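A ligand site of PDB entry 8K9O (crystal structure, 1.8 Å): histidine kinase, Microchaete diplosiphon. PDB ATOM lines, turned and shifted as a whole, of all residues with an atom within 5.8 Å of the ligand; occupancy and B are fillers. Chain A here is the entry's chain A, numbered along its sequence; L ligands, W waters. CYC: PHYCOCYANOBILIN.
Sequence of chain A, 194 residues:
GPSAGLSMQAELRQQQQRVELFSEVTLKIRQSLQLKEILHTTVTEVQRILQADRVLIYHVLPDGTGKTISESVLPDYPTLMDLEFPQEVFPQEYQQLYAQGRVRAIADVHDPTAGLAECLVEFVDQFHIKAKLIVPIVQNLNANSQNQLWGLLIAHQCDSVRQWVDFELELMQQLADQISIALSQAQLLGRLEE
SG of Cys 119 is covalently linked to CAC of the ligand, at 1.8 Å.
The side-chain hydroxyl (OH) of Tyr 98 sits at hydrogen-bond distance from an oxygen (O1A) of the ligand (2.6 Å).
OB of the ligand is in hydrogen-bond range of NE2 of His 156 (2.7 Å).
The backbone carbonyl oxygen of Val 89 lies within hydrogen-bond range of a nitrogen (NC) of the ligand, 3.2 Å away.
An oxygen (O1A) of the ligand lies within salt-bridge range of the guanidinium group (NE) of Arg 102 (2.8 Å).
An oxygen (O1D) of the ligand is in hydrogen-bond range of the backbone NH (N) of Ala 117.
NH2 of Arg 104 is in salt-bridge range of O2A of the ligand (2.9 Å).
O of Arg 104 lies within hydrogen-bond range of N of Ile 134.
N of Ile 106 lies within hydrogen-bond range of O of Lys 132.
The backbone NH (N) of Ile 154 sits at hydrogen-bond distance from the backbone carbonyl oxygen (O) of Leu 56 (2.9 Å).
N of Leu 152 lies within hydrogen-bond range of O of Tyr 58 (2.8 Å).
The backbone carbonyl oxygen of Val 124 lies within hydrogen-bond range of the backbone NH of Ile 129 (3.2 Å).
NZ of Lys 132 lies close to NB of the ligand (3.1 Å).
Leu 80 touches the ligand.
Glu 88 touches the ligand.
CD1 of Phe 90 touches C2A of the ligand (3.6 Å).
Pro 91 touches the ligand (CD to ND, 3.4 Å).
CE1 of Tyr 94 touches CAD of the ligand, at 3.5 Å.
Gly 115 touches the ligand.
Leu 116 touches the ligand (CA to O1D, 3.4 Å).
Leu 120 touches the ligand.
Phe 123 touches the ligand.
Ile 129 touches the ligand.
Leu 152 touches the ligand (CD1 to CMA, 3.95 Å).
CG2 of Ile 154 touches OB of the ligand (3.8 Å).
Hydrophobic or aromatic side chains within 4 Å of the ligand: Leu 80, Val 89, Phe 90, Pro 91, Tyr 94, Tyr 98, Ala 117, Leu 120, Phe 123, Ile 129, Leu 152, Ile 154 and His 156.
Of the 28 residues printed, 20 come within 4 Å of the ligand.
Along chain A the residues within 4 Å of the ligand span positions 80 to 156.
The nearest printed residue that does not touch the ligand is Tyr 58 (4.01 Å).
Water W2 lies within hydrogen-bond range of O1D of the ligand and NH2 of Arg 104.
Water W1 lies within hydrogen-bond range of the backbone carbonyl oxygen of Gly 115 (2.5 Å), an oxygen (O2D) of the ligand (2.7 Å) and the backbone NH of Ala 117 (3.1 Å).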
ATOM      1  N   LEU A  56       7.316 -15.410 -21.731  1.00  0.00           N
ATOM      2  CA  LEU A  56       8.778 -15.132 -21.639  1.00  0.00           C
ATOM      3  C   LEU A  56       9.511 -15.976 -22.666  1.00  0.00           C
ATOM      4  O   LEU A  56       8.950 -16.982 -23.217  1.00  0.00           O
ATOM      5  CB  LEU A  56       9.235 -15.441 -20.219  1.00  0.00           C
ATOM      6  CG  LEU A  56       9.136 -16.924 -19.850  1.00  0.00           C
ATOM      7  CD1 LEU A  56      10.445 -17.660 -19.848  1.00  0.00           C
ATOM      8  CD2 LEU A  56       8.456 -17.078 -18.533  1.00  0.00           C
ATOM      9  N   TYR A  58      13.007 -18.074 -22.520  1.00  0.00           N
ATOM     10  CA  TYR A  58      14.047 -18.666 -21.642  1.00  0.00           C
ATOM     11  C   TYR A  58      15.165 -19.179 -22.543  1.00  0.00           C
ATOM     12  O   TYR A  58      14.937 -20.046 -23.362  1.00  0.00           O
ATOM     13  CB  TYR A  58      13.382 -19.744 -20.793  1.00  0.00           C
ATOM     14  CG  TYR A  58      14.276 -20.338 -19.735  1.00  0.00           C
ATOM     15  CD1 TYR A  58      14.518 -19.661 -18.560  1.00  0.00           C
ATOM     16  CD2 TYR A  58      14.876 -21.584 -19.915  1.00  0.00           C
ATOM     17  CE1 TYR A  58      15.335 -20.175 -17.571  1.00  0.00           C
ATOM     18  CE2 TYR A  58      15.689 -22.122 -18.929  1.00  0.00           C
ATOM     19  CZ  TYR A  58      15.920 -21.407 -17.771  1.00  0.00           C
ATOM     20  OH  TYR A  58      16.721 -21.929 -16.796  1.00  0.00           O
ATOM     21  N   LEU A  80      10.526 -13.053 -13.757  1.00  0.00           N
ATOM     22  CA  LEU A  80      11.682 -13.951 -13.950  1.00  0.00           C
ATOM     23  C   LEU A  80      12.833 -13.251 -14.658  1.00  0.00           C
ATOM     24  O   LEU A  80      13.860 -13.903 -14.899  1.00  0.00           O
ATOM     25  CB  LEU A  80      11.191 -15.169 -14.738  1.00  0.00           C
ATOM     26  CG  LEU A  80      10.308 -16.103 -13.908  1.00  0.00           C
ATOM     27  CD1 LEU A  80       9.275 -16.835 -14.723  1.00  0.00           C
ATOM     28  CD2 LEU A  80      11.176 -17.088 -13.157  1.00  0.00           C
ATOM     29  N   PHE A  85      19.227 -19.759 -13.689  1.00  0.00           N
ATOM     30  CA  PHE A  85      18.933 -21.070 -13.057  1.00  0.00           C
ATOM     31  C   PHE A  85      19.931 -22.087 -13.543  1.00  0.00           C
ATOM     32  O   PHE A  85      20.434 -22.012 -14.659  1.00  0.00           O
ATOM     33  CB  PHE A  85      17.532 -21.573 -13.367  1.00  0.00           C
ATOM     34  CG  PHE A  85      16.448 -20.671 -12.882  1.00  0.00           C
ATOM     35  CD1 PHE A  85      16.244 -20.474 -11.525  1.00  0.00           C
ATOM     36  CD2 PHE A  85      15.635 -20.005 -13.791  1.00  0.00           C
ATOM     37  CE1 PHE A  85      15.236 -19.619 -11.090  1.00  0.00           C
ATOM     38  CE2 PHE A  85      14.630 -19.170 -13.342  1.00  0.00           C
ATOM     39  CZ  PHE A  85      14.435 -18.981 -11.997  1.00  0.00           C
ATOM     40  N   GLU A  88      19.568 -28.119 -13.361  1.00  0.00           N
ATOM     41  CA  GLU A  88      18.569 -29.022 -12.716  1.00  0.00           C
ATOM     42  C   GLU A  88      17.133 -28.510 -12.885  1.00  0.00           C
ATOM     43  O   GLU A  88      16.215 -29.327 -12.725  1.00  0.00           O
ATOM     44  CB  GLU A  88      18.827 -29.214 -11.227  1.00  0.00           C
ATOM     45  CG  GLU A  88      18.682 -27.948 -10.378  1.00  0.00           C
ATOM     46  CD  GLU A  88      18.546 -28.178  -8.878  1.00  0.00           C
ATOM     47  OE1 GLU A  88      18.208 -29.324  -8.494  1.00  0.00           O
ATOM     48  OE2 GLU A  88      18.711 -27.209  -8.084  1.00  0.00           O
ATOM     49  N   VAL A  89      16.878 -27.221 -13.117  1.00  0.00           N
ATOM     50  CA  VAL A  89      15.452 -26.779 -13.272  1.00  0.00           C
ATOM     51  C   VAL A  89      14.871 -27.269 -14.606  1.00  0.00           C
ATOM     52  O   VAL A  89      13.629 -27.251 -14.764  1.00  0.00           O
ATOM     53  CB  VAL A  89      15.238 -25.261 -13.128  1.00  0.00           C
ATOM     54  CG1 VAL A  89      15.766 -24.750 -11.789  1.00  0.00           C
ATOM     55  CG2 VAL A  89      15.772 -24.488 -14.286  1.00  0.00           C
ATOM     56  N   PHE A  90      15.707 -27.656 -15.552  1.00  0.00           N
ATOM     57  CA  PHE A  90      15.313 -28.069 -16.926  1.00  0.00           C
ATOM     58  C   PHE A  90      16.393 -29.008 -17.422  1.00  0.00           C
ATOM     59  O   PHE A  90      17.285 -28.606 -18.146  1.00  0.00           O
ATOM     60  CB  PHE A  90      15.027 -26.833 -17.785  1.00  0.00           C
ATOM     61  CG  PHE A  90      14.613 -27.107 -19.211  1.00  0.00           C
ATOM     62  CD1 PHE A  90      13.646 -28.063 -19.471  1.00  0.00           C
ATOM     63  CD2 PHE A  90      15.090 -26.358 -20.263  1.00  0.00           C
ATOM     64  CE1 PHE A  90      13.261 -28.323 -20.779  1.00  0.00           C
ATOM     65  CE2 PHE A  90      14.641 -26.558 -21.561  1.00  0.00           C
ATOM     66  CZ  PHE A  90      13.742 -27.572 -21.822  1.00  0.00           C
ATOM     67  N   PRO A  91      16.283 -30.286 -17.037  1.00  0.00           N
ATOM     68  CA  PRO A  91      17.340 -31.266 -17.302  1.00  0.00           C
ATOM     69  C   PRO A  91      17.744 -31.421 -18.772  1.00  0.00           C
ATOM     70  O   PRO A  91      16.902 -31.404 -19.696  1.00  0.00           O
ATOM     71  CB  PRO A  91      16.743 -32.577 -16.783  1.00  0.00           C
ATOM     72  CG  PRO A  91      15.739 -32.178 -15.763  1.00  0.00           C
ATOM     73  CD  PRO A  91      15.188 -30.854 -16.232  1.00  0.00           C
ATOM     74  N   TYR A  94      15.741 -33.470 -21.178  1.00  0.00           N
ATOM     75  CA  TYR A  94      14.515 -32.801 -21.682  1.00  0.00           C
ATOM     76  C   TYR A  94      14.913 -31.674 -22.650  1.00  0.00           C
ATOM     77  O   TYR A  94      14.199 -31.499 -23.644  1.00  0.00           O
ATOM     78  CB  TYR A  94      13.617 -32.397 -20.517  1.00  0.00           C
ATOM     79  CG  TYR A  94      12.670 -33.500 -20.137  1.00  0.00           C
ATOM     80  CD1 TYR A  94      13.151 -34.620 -19.507  1.00  0.00           C
ATOM     81  CD2 TYR A  94      11.324 -33.468 -20.468  1.00  0.00           C
ATOM     82  CE1 TYR A  94      12.330 -35.673 -19.168  1.00  0.00           C
ATOM     83  CE2 TYR A  94      10.488 -34.529 -20.143  1.00  0.00           C
ATOM     84  CZ  TYR A  94      11.012 -35.655 -19.550  1.00  0.00           C
ATOM     85  OH  TYR A  94      10.270 -36.748 -19.176  1.00  0.00           O
ATOM     86  N   TYR A  98      13.281 -31.303 -26.436  1.00  0.00           N
ATOM     87  CA  TYR A  98      12.800 -29.999 -26.972  1.00  0.00           C
ATOM     88  C   TYR A  98      13.546 -29.684 -28.269  1.00  0.00           C
ATOM     89  O   TYR A  98      12.940 -29.220 -29.251  1.00  0.00           O
ATOM     90  CB  TYR A  98      12.827 -28.878 -25.909  1.00  0.00           C
ATOM     91  CG  TYR A  98      11.610 -28.911 -25.010  1.00  0.00           C
ATOM     92  CD1 TYR A  98      10.446 -28.235 -25.385  1.00  0.00           C
ATOM     93  CD2 TYR A  98      11.563 -29.636 -23.834  1.00  0.00           C
ATOM     94  CE1 TYR A  98       9.293 -28.296 -24.616  1.00  0.00           C
ATOM     95  CE2 TYR A  98      10.409 -29.651 -23.032  1.00  0.00           C
ATOM     96  CZ  TYR A  98       9.263 -29.004 -23.440  1.00  0.00           C
ATOM     97  OH  TYR A  98       8.154 -29.055 -22.646  1.00  0.00           O
ATOM     98  N   ARG A 102       9.713 -31.479 -28.959  1.00  0.00           N
ATOM     99  CA  ARG A 102       8.750 -31.654 -27.846  1.00  0.00           C
ATOM    100  C   ARG A 102       7.998 -30.328 -27.627  1.00  0.00           C
ATOM    101  O   ARG A 102       8.644 -29.272 -27.721  1.00  0.00           O
ATOM    102  CB  ARG A 102       9.415 -32.117 -26.556  1.00  0.00           C
ATOM    103  CG  ARG A 102       8.427 -32.290 -25.422  1.00  0.00           C
ATOM    104  CD  ARG A 102       9.117 -32.995 -24.265  1.00  0.00           C
ATOM    105  NE  ARG A 102       8.343 -33.114 -23.065  1.00  0.00           N
ATOM    106  CZ  ARG A 102       7.469 -34.087 -22.793  1.00  0.00           C
ATOM    107  NH1 ARG A 102       7.168 -35.027 -23.696  1.00  0.00           N
ATOM    108  NH2 ARG A 102       6.898 -34.132 -21.625  1.00  0.00           N
ATOM    109  N   VAL A 103       6.697 -30.383 -27.366  1.00  0.00           N
ATOM    110  CA  VAL A 103       5.900 -29.223 -26.863  1.00  0.00           C
ATOM    111  C   VAL A 103       5.137 -29.684 -25.642  1.00  0.00           C
ATOM    112  O   VAL A 103       4.911 -30.916 -25.501  1.00  0.00           O
ATOM    113  CB  VAL A 103       4.962 -28.661 -27.939  1.00  0.00           C
ATOM    114  CG1 VAL A 103       5.717 -28.158 -29.147  1.00  0.00           C
ATOM    115  CG2 VAL A 103       3.903 -29.700 -28.308  1.00  0.00           C
ATOM    116  N   ARG A 104       4.678 -28.763 -24.810  1.00  0.00           N
ATOM    117  CA  ARG A 104       3.772 -29.122 -23.703  1.00  0.00           C
ATOM    118  C   ARG A 104       2.706 -28.054 -23.624  1.00  0.00           C
ATOM    119  O   ARG A 104       3.052 -26.881 -23.664  1.00  0.00           O
ATOM    120  CB  ARG A 104       4.371 -29.163 -22.289  1.00  0.00           C
ATOM    121  CG  ARG A 104       5.123 -30.407 -21.877  1.00  0.00           C
ATOM    122  CD  ARG A 104       4.449 -31.742 -22.052  1.00  0.00           C
ATOM    123  NE  ARG A 104       3.288 -32.044 -21.248  1.00  0.00           N
ATOM    124  CZ  ARG A 104       3.310 -32.528 -20.031  1.00  0.00           C
ATOM    125  NH1 ARG A 104       2.174 -32.817 -19.428  1.00  0.00           N
ATOM    126  NH2 ARG A 104       4.448 -32.720 -19.409  1.00  0.00           N
ATOM    127  N   ILE A 106       0.028 -27.540 -20.635  1.00  0.00           N
ATOM    128  CA  ILE A 106      -0.427 -28.067 -19.318  1.00  0.00           C
ATOM    129  C   ILE A 106      -1.471 -27.128 -18.747  1.00  0.00           C
ATOM    130  O   ILE A 106      -1.112 -25.989 -18.407  1.00  0.00           O
ATOM    131  CB  ILE A 106       0.773 -28.289 -18.380  1.00  0.00           C
ATOM    132  CG1 ILE A 106       1.760 -29.309 -18.961  1.00  0.00           C
ATOM    133  CG2 ILE A 106       0.313 -28.678 -16.965  1.00  0.00           C
ATOM    134  CD1 ILE A 106       3.185 -29.109 -18.502  1.00  0.00           C
ATOM    135  N   GLY A 115       1.650 -35.318 -14.732  1.00  0.00           N
ATOM    136  CA  GLY A 115       2.888 -36.125 -14.572  1.00  0.00           C
ATOM    137  C   GLY A 115       4.125 -35.305 -14.205  1.00  0.00           C
ATOM    138  O   GLY A 115       5.224 -35.812 -14.403  1.00  0.00           O
ATOM    139  N   LEU A 116       3.978 -34.065 -13.736  1.00  0.00           N
ATOM    140  CA  LEU A 116       5.175 -33.199 -13.509  1.00  0.00           C
ATOM    141  C   LEU A 116       5.907 -33.702 -12.256  1.00  0.00           C
ATOM    142  O   LEU A 116       5.215 -33.988 -11.232  1.00  0.00           O
ATOM    143  CB  LEU A 116       4.745 -31.737 -13.320  1.00  0.00           C
ATOM    144  CG  LEU A 116       4.406 -30.946 -14.583  1.00  0.00           C
ATOM    145  CD1 LEU A 116       3.239 -31.576 -15.328  1.00  0.00           C
ATOM    146  CD2 LEU A 116       4.102 -29.498 -14.197  1.00  0.00           C
ATOM    147  N   ALA A 117       7.237 -33.727 -12.331  1.00  0.00           N
ATOM    148  CA  ALA A 117       8.132 -33.893 -11.155  1.00  0.00           C
ATOM    149  C   ALA A 117       7.603 -33.047  -9.999  1.00  0.00           C
ATOM    150  O   ALA A 117       7.216 -31.881 -10.235  1.00  0.00           O
ATOM    151  CB  ALA A 117       9.512 -33.498 -11.517  1.00  0.00           C
ATOM    152  N   CYS A 119       9.352 -31.663  -7.691  1.00  0.00           N
ATOM    153  CA  CYS A 119      10.276 -30.497  -7.547  1.00  0.00           C
ATOM    154  C   CYS A 119       9.972 -29.420  -8.612  1.00  0.00           C
ATOM    155  O   CYS A 119      10.055 -28.217  -8.302  1.00  0.00           O
ATOM    156  CB  CYS A 119      11.727 -30.938  -7.602  1.00  0.00           C
ATOM    157  SG  CYS A 119      12.238 -31.657  -9.173  1.00  0.00           S
ATOM    158  N   LEU A 120       9.538 -29.854  -9.798  1.00  0.00           N
ATOM    159  CA  LEU A 120       9.111 -28.907 -10.879  1.00  0.00           C
ATOM    160  C   LEU A 120       7.811 -28.207 -10.510  1.00  0.00           C
ATOM    161  O   LEU A 120       7.688 -26.951 -10.764  1.00  0.00           O
ATOM    162  CB  LEU A 120       8.997 -29.654 -12.208  1.00  0.00           C
ATOM    163  CG  LEU A 120       8.468 -28.793 -13.370  1.00  0.00           C
ATOM    164  CD1 LEU A 120       9.376 -27.585 -13.630  1.00  0.00           C
ATOM    165  CD2 LEU A 120       8.344 -29.635 -14.625  1.00  0.00           C
ATOM    166  N   PHE A 123       8.782 -25.577  -8.118  1.00  0.00           N
ATOM    167  CA  PHE A 123       9.519 -24.485  -8.811  1.00  0.00           C
ATOM    168  C   PHE A 123       8.509 -23.551  -9.459  1.00  0.00           C
ATOM    169  O   PHE A 123       8.545 -22.345  -9.242  1.00  0.00           O
ATOM    170  CB  PHE A 123      10.495 -25.069  -9.814  1.00  0.00           C
ATOM    171  CG  PHE A 123      11.226 -24.034 -10.612  1.00  0.00           C
ATOM    172  CD1 PHE A 123      12.183 -23.236 -10.017  1.00  0.00           C
ATOM    173  CD2 PHE A 123      10.876 -23.810 -11.929  1.00  0.00           C
ATOM    174  CE1 PHE A 123      12.844 -22.279 -10.755  1.00  0.00           C
ATOM    175  CE2 PHE A 123      11.538 -22.844 -12.680  1.00  0.00           C
ATOM    176  CZ  PHE A 123      12.527 -22.097 -12.085  1.00  0.00           C
ATOM    177  N   VAL A 124       7.561 -24.088 -10.216  1.00  0.00           N
ATOM    178  CA  VAL A 124       6.613 -23.191 -10.957  1.00  0.00           C
ATOM    179  C   VAL A 124       5.711 -22.475  -9.940  1.00  0.00           C
ATOM    180  O   VAL A 124       5.292 -21.312 -10.174  1.00  0.00           O
ATOM    181  CB  VAL A 124       5.882 -23.923 -12.091  1.00  0.00           C
ATOM    182  CG1 VAL A 124       6.851 -24.418 -13.160  1.00  0.00           C
ATOM    183  CG2 VAL A 124       4.954 -25.020 -11.620  1.00  0.00           C
ATOM    184  N   PHE A 127       6.522 -18.898  -8.901  1.00  0.00           N
ATOM    185  CA  PHE A 127       6.100 -17.816  -9.843  1.00  0.00           C
ATOM    186  C   PHE A 127       4.555 -17.796  -9.993  1.00  0.00           C
ATOM    187  O   PHE A 127       4.114 -17.106 -10.944  1.00  0.00           O
ATOM    188  CB  PHE A 127       6.918 -17.970 -11.121  1.00  0.00           C
ATOM    189  CG  PHE A 127       8.368 -18.200 -10.801  1.00  0.00           C
ATOM    190  CD1 PHE A 127       9.087 -17.204 -10.154  1.00  0.00           C
ATOM    191  CD2 PHE A 127       8.985 -19.423 -11.049  1.00  0.00           C
ATOM    192  CE1 PHE A 127      10.417 -17.405  -9.794  1.00  0.00           C
ATOM    193  CE2 PHE A 127      10.316 -19.614 -10.703  1.00  0.00           C
ATOM    194  CZ  PHE A 127      11.032 -18.611 -10.079  1.00  0.00           C
ATOM    195  N   ILE A 129       2.509 -20.028 -10.938  1.00  0.00           N
ATOM    196  CA  ILE A 129       2.099 -20.658 -12.225  1.00  0.00           C
ATOM    197  C   ILE A 129       1.048 -21.739 -11.943  1.00  0.00           C
ATOM    198  O   ILE A 129       1.313 -22.612 -11.083  1.00  0.00           O
ATOM    199  CB  ILE A 129       3.325 -21.207 -12.960  1.00  0.00           C
ATOM    200  CG1 ILE A 129       4.255 -20.072 -13.398  1.00  0.00           C
ATOM    201  CG2 ILE A 129       2.912 -22.059 -14.165  1.00  0.00           C
ATOM    202  CD1 ILE A 129       5.697 -20.456 -13.619  1.00  0.00           C
ATOM    203  N   LYS A 132       0.882 -23.901 -18.034  1.00  0.00           N
ATOM    204  CA  LYS A 132       2.042 -23.504 -18.863  1.00  0.00           C
ATOM    205  C   LYS A 132       1.990 -24.142 -20.244  1.00  0.00           C
ATOM    206  O   LYS A 132       1.541 -25.290 -20.392  1.00  0.00           O
ATOM    207  CB  LYS A 132       3.366 -23.761 -18.153  1.00  0.00           C
ATOM    208  CG  LYS A 132       3.787 -25.203 -17.989  1.00  0.00           C
ATOM    209  CD  LYS A 132       5.066 -25.256 -17.117  1.00  0.00           C
ATOM    210  CE  LYS A 132       5.881 -26.500 -17.338  1.00  0.00           C
ATOM    211  NZ  LYS A 132       7.105 -26.503 -16.491  1.00  0.00           N
ATOM    212  N   ILE A 134       4.588 -24.516 -23.572  1.00  0.00           N
ATOM    213  CA  ILE A 134       6.053 -24.595 -23.796  1.00  0.00           C
ATOM    214  C   ILE A 134       6.341 -25.003 -25.218  1.00  0.00           C
ATOM    215  O   ILE A 134       5.926 -26.097 -25.637  1.00  0.00           O
ATOM    216  CB  ILE A 134       6.769 -25.581 -22.829  1.00  0.00           C
ATOM    217  CG1 ILE A 134       6.231 -25.498 -21.399  1.00  0.00           C
ATOM    218  CG2 ILE A 134       8.279 -25.378 -22.936  1.00  0.00           C
ATOM    219  CD1 ILE A 134       6.573 -24.244 -20.695  1.00  0.00           C
ATOM    220  N   LEU A 152      13.234 -21.528 -24.987  1.00  0.00           N
ATOM    221  CA  LEU A 152      11.801 -21.885 -24.892  1.00  0.00           C
ATOM    222  C   LEU A 152      11.015 -20.583 -24.996  1.00  0.00           C
ATOM    223  O   LEU A 152      11.424 -19.587 -24.427  1.00  0.00           O
ATOM    224  CB  LEU A 152      11.475 -22.586 -23.568  1.00  0.00           C
ATOM    225  CG  LEU A 152      12.246 -23.876 -23.272  1.00  0.00           C
ATOM    226  CD1 LEU A 152      11.929 -24.346 -21.870  1.00  0.00           C
ATOM    227  CD2 LEU A 152      11.965 -24.920 -24.334  1.00  0.00           C
ATOM    228  N   ILE A 154       7.453 -19.440 -23.754  1.00  0.00           N
ATOM    229  CA  ILE A 154       6.591 -19.967 -22.664  1.00  0.00           C
ATOM    230  C   ILE A 154       5.466 -18.991 -22.371  1.00  0.00           C
ATOM    231  O   ILE A 154       5.721 -17.806 -22.322  1.00  0.00           O
ATOM    232  CB  ILE A 154       7.435 -20.247 -21.416  1.00  0.00           C
ATOM    233  CG1 ILE A 154       8.574 -21.231 -21.735  1.00  0.00           C
ATOM    234  CG2 ILE A 154       6.585 -20.651 -20.230  1.00  0.00           C
ATOM    235  CD1 ILE A 154       9.486 -21.461 -20.504  1.00  0.00           C
ATOM    236  N   HIS A 156       2.382 -18.587 -19.380  1.00  0.00           N
ATOM    237  CA  HIS A 156       1.847 -19.030 -18.088  1.00  0.00           C
ATOM    238  C   HIS A 156       0.497 -18.385 -17.838  1.00  0.00           C
ATOM    239  O   HIS A 156       0.346 -17.164 -18.105  1.00  0.00           O
ATOM    240  CB  HIS A 156       2.722 -18.645 -16.885  1.00  0.00           C
ATOM    241  CG  HIS A 156       4.115 -19.188 -16.946  1.00  0.00           C
ATOM    242  ND1 HIS A 156       5.187 -18.453 -16.501  1.00  0.00           N
ATOM    243  CD2 HIS A 156       4.597 -20.411 -17.274  1.00  0.00           C
ATOM    244  CE1 HIS A 156       6.286 -19.153 -16.658  1.00  0.00           C
ATOM    245  NE2 HIS A 156       5.956 -20.387 -17.085  1.00  0.00           N
HETATM  246  CHA CYC L   1      11.179 -30.420 -16.817  1.00  0.00           C
HETATM  247  NA  CYC L   1      11.422 -27.992 -16.310  1.00  0.00           N
HETATM  248  C1A CYC L   1      10.980 -29.054 -17.070  1.00  0.00           C
HETATM  249  C2A CYC L   1      10.264 -28.581 -18.243  1.00  0.00           C
HETATM  250  C3A CYC L   1      10.270 -27.228 -18.187  1.00  0.00           C
HETATM  251  C4A CYC L   1      10.995 -26.850 -16.956  1.00  0.00           C
HETATM  252  CMA CYC L   1       9.725 -26.272 -19.213  1.00  0.00           C
HETATM  253  CAA CYC L   1       9.689 -29.500 -19.300  1.00  0.00           C
HETATM  254  CBA CYC L   1       8.375 -30.160 -18.916  1.00  0.00           C
HETATM  255  CGA CYC L   1       7.924 -31.246 -19.877  1.00  0.00           C
HETATM  256  O1A CYC L   1       8.196 -31.082 -21.080  1.00  0.00           O
HETATM  257  O2A CYC L   1       7.361 -32.285 -19.410  1.00  0.00           O
HETATM  258  CHB CYC L   1      11.243 -25.563 -16.512  1.00  0.00           C
HETATM  259  NB  CYC L   1       9.165 -24.290 -17.030  1.00  0.00           N
HETATM  260  C1B CYC L   1      10.520 -24.392 -16.662  1.00  0.00           C
HETATM  261  C2B CYC L   1      11.034 -23.094 -16.502  1.00  0.00           C
HETATM  262  C3B CYC L   1      10.018 -22.202 -16.650  1.00  0.00           C
HETATM  263  C4B CYC L   1       8.775 -22.967 -16.986  1.00  0.00           C
HETATM  264  CMB CYC L   1      12.464 -22.723 -16.213  1.00  0.00           C
HETATM  265  CAB CYC L   1      10.032 -20.720 -16.431  1.00  0.00           C
HETATM  266  CBB CYC L   1       9.373 -20.373 -15.113  1.00  0.00           C
HETATM  267  OB  CYC L   1       7.627 -22.563 -17.085  1.00  0.00           O
HETATM  268  NC  CYC L   1      12.750 -28.932 -12.196  1.00  0.00           N
HETATM  269  C1C CYC L   1      12.804 -27.975 -11.255  1.00  0.00           C
HETATM  270  C2C CYC L   1      13.382 -28.575  -9.982  1.00  0.00           C
HETATM  271  C3C CYC L   1      14.041 -29.880 -10.469  1.00  0.00           C
HETATM  272  C4C CYC L   1      13.364 -30.116 -11.801  1.00  0.00           C
HETATM  273  CMC CYC L   1      14.309 -27.625  -9.261  1.00  0.00           C
HETATM  274  CAC CYC L   1      13.946 -31.086  -9.522  1.00  0.00           C
HETATM  275  CBC CYC L   1      14.721 -30.836  -8.244  1.00  0.00           C
HETATM  276  OC  CYC L   1      12.454 -26.820 -11.426  1.00  0.00           O
HETATM  277  CHD CYC L   1      13.326 -31.282 -12.493  1.00  0.00           C
HETATM  278  ND  CYC L   1      12.214 -30.532 -14.581  1.00  0.00           N
HETATM  279  C1D CYC L   1      12.693 -31.502 -13.747  1.00  0.00           C
HETATM  280  C2D CYC L   1      12.461 -32.768 -14.380  1.00  0.00           C
HETATM  281  C3D CYC L   1      11.817 -32.526 -15.564  1.00  0.00           C
HETATM  282  C4D CYC L   1      11.698 -31.095 -15.723  1.00  0.00           C
HETATM  283  CMD CYC L   1      12.780 -34.104 -13.794  1.00  0.00           C
HETATM  284  CAD CYC L   1      11.377 -33.568 -16.564  1.00  0.00           C
HETATM  285  CBD CYC L   1       9.865 -33.738 -16.675  1.00  0.00           C
HETATM  286  CGD CYC L   1       9.136 -34.214 -15.419  1.00  0.00           C
HETATM  287  O1D CYC L   1       8.134 -33.583 -15.049  1.00  0.00           O
HETATM  288  O2D CYC L   1       9.598 -35.189 -14.787  1.00  0.00           O
HETATM  289  O   HOH W   1       7.544 -36.500 -13.660  1.00  0.00           O
HETATM  290  O   HOH W   2       6.899 -33.763 -17.272  1.00  0.00           O
HETATM  291  O   HOH W   3      11.064 -37.108 -15.716  1.00  0.00           O
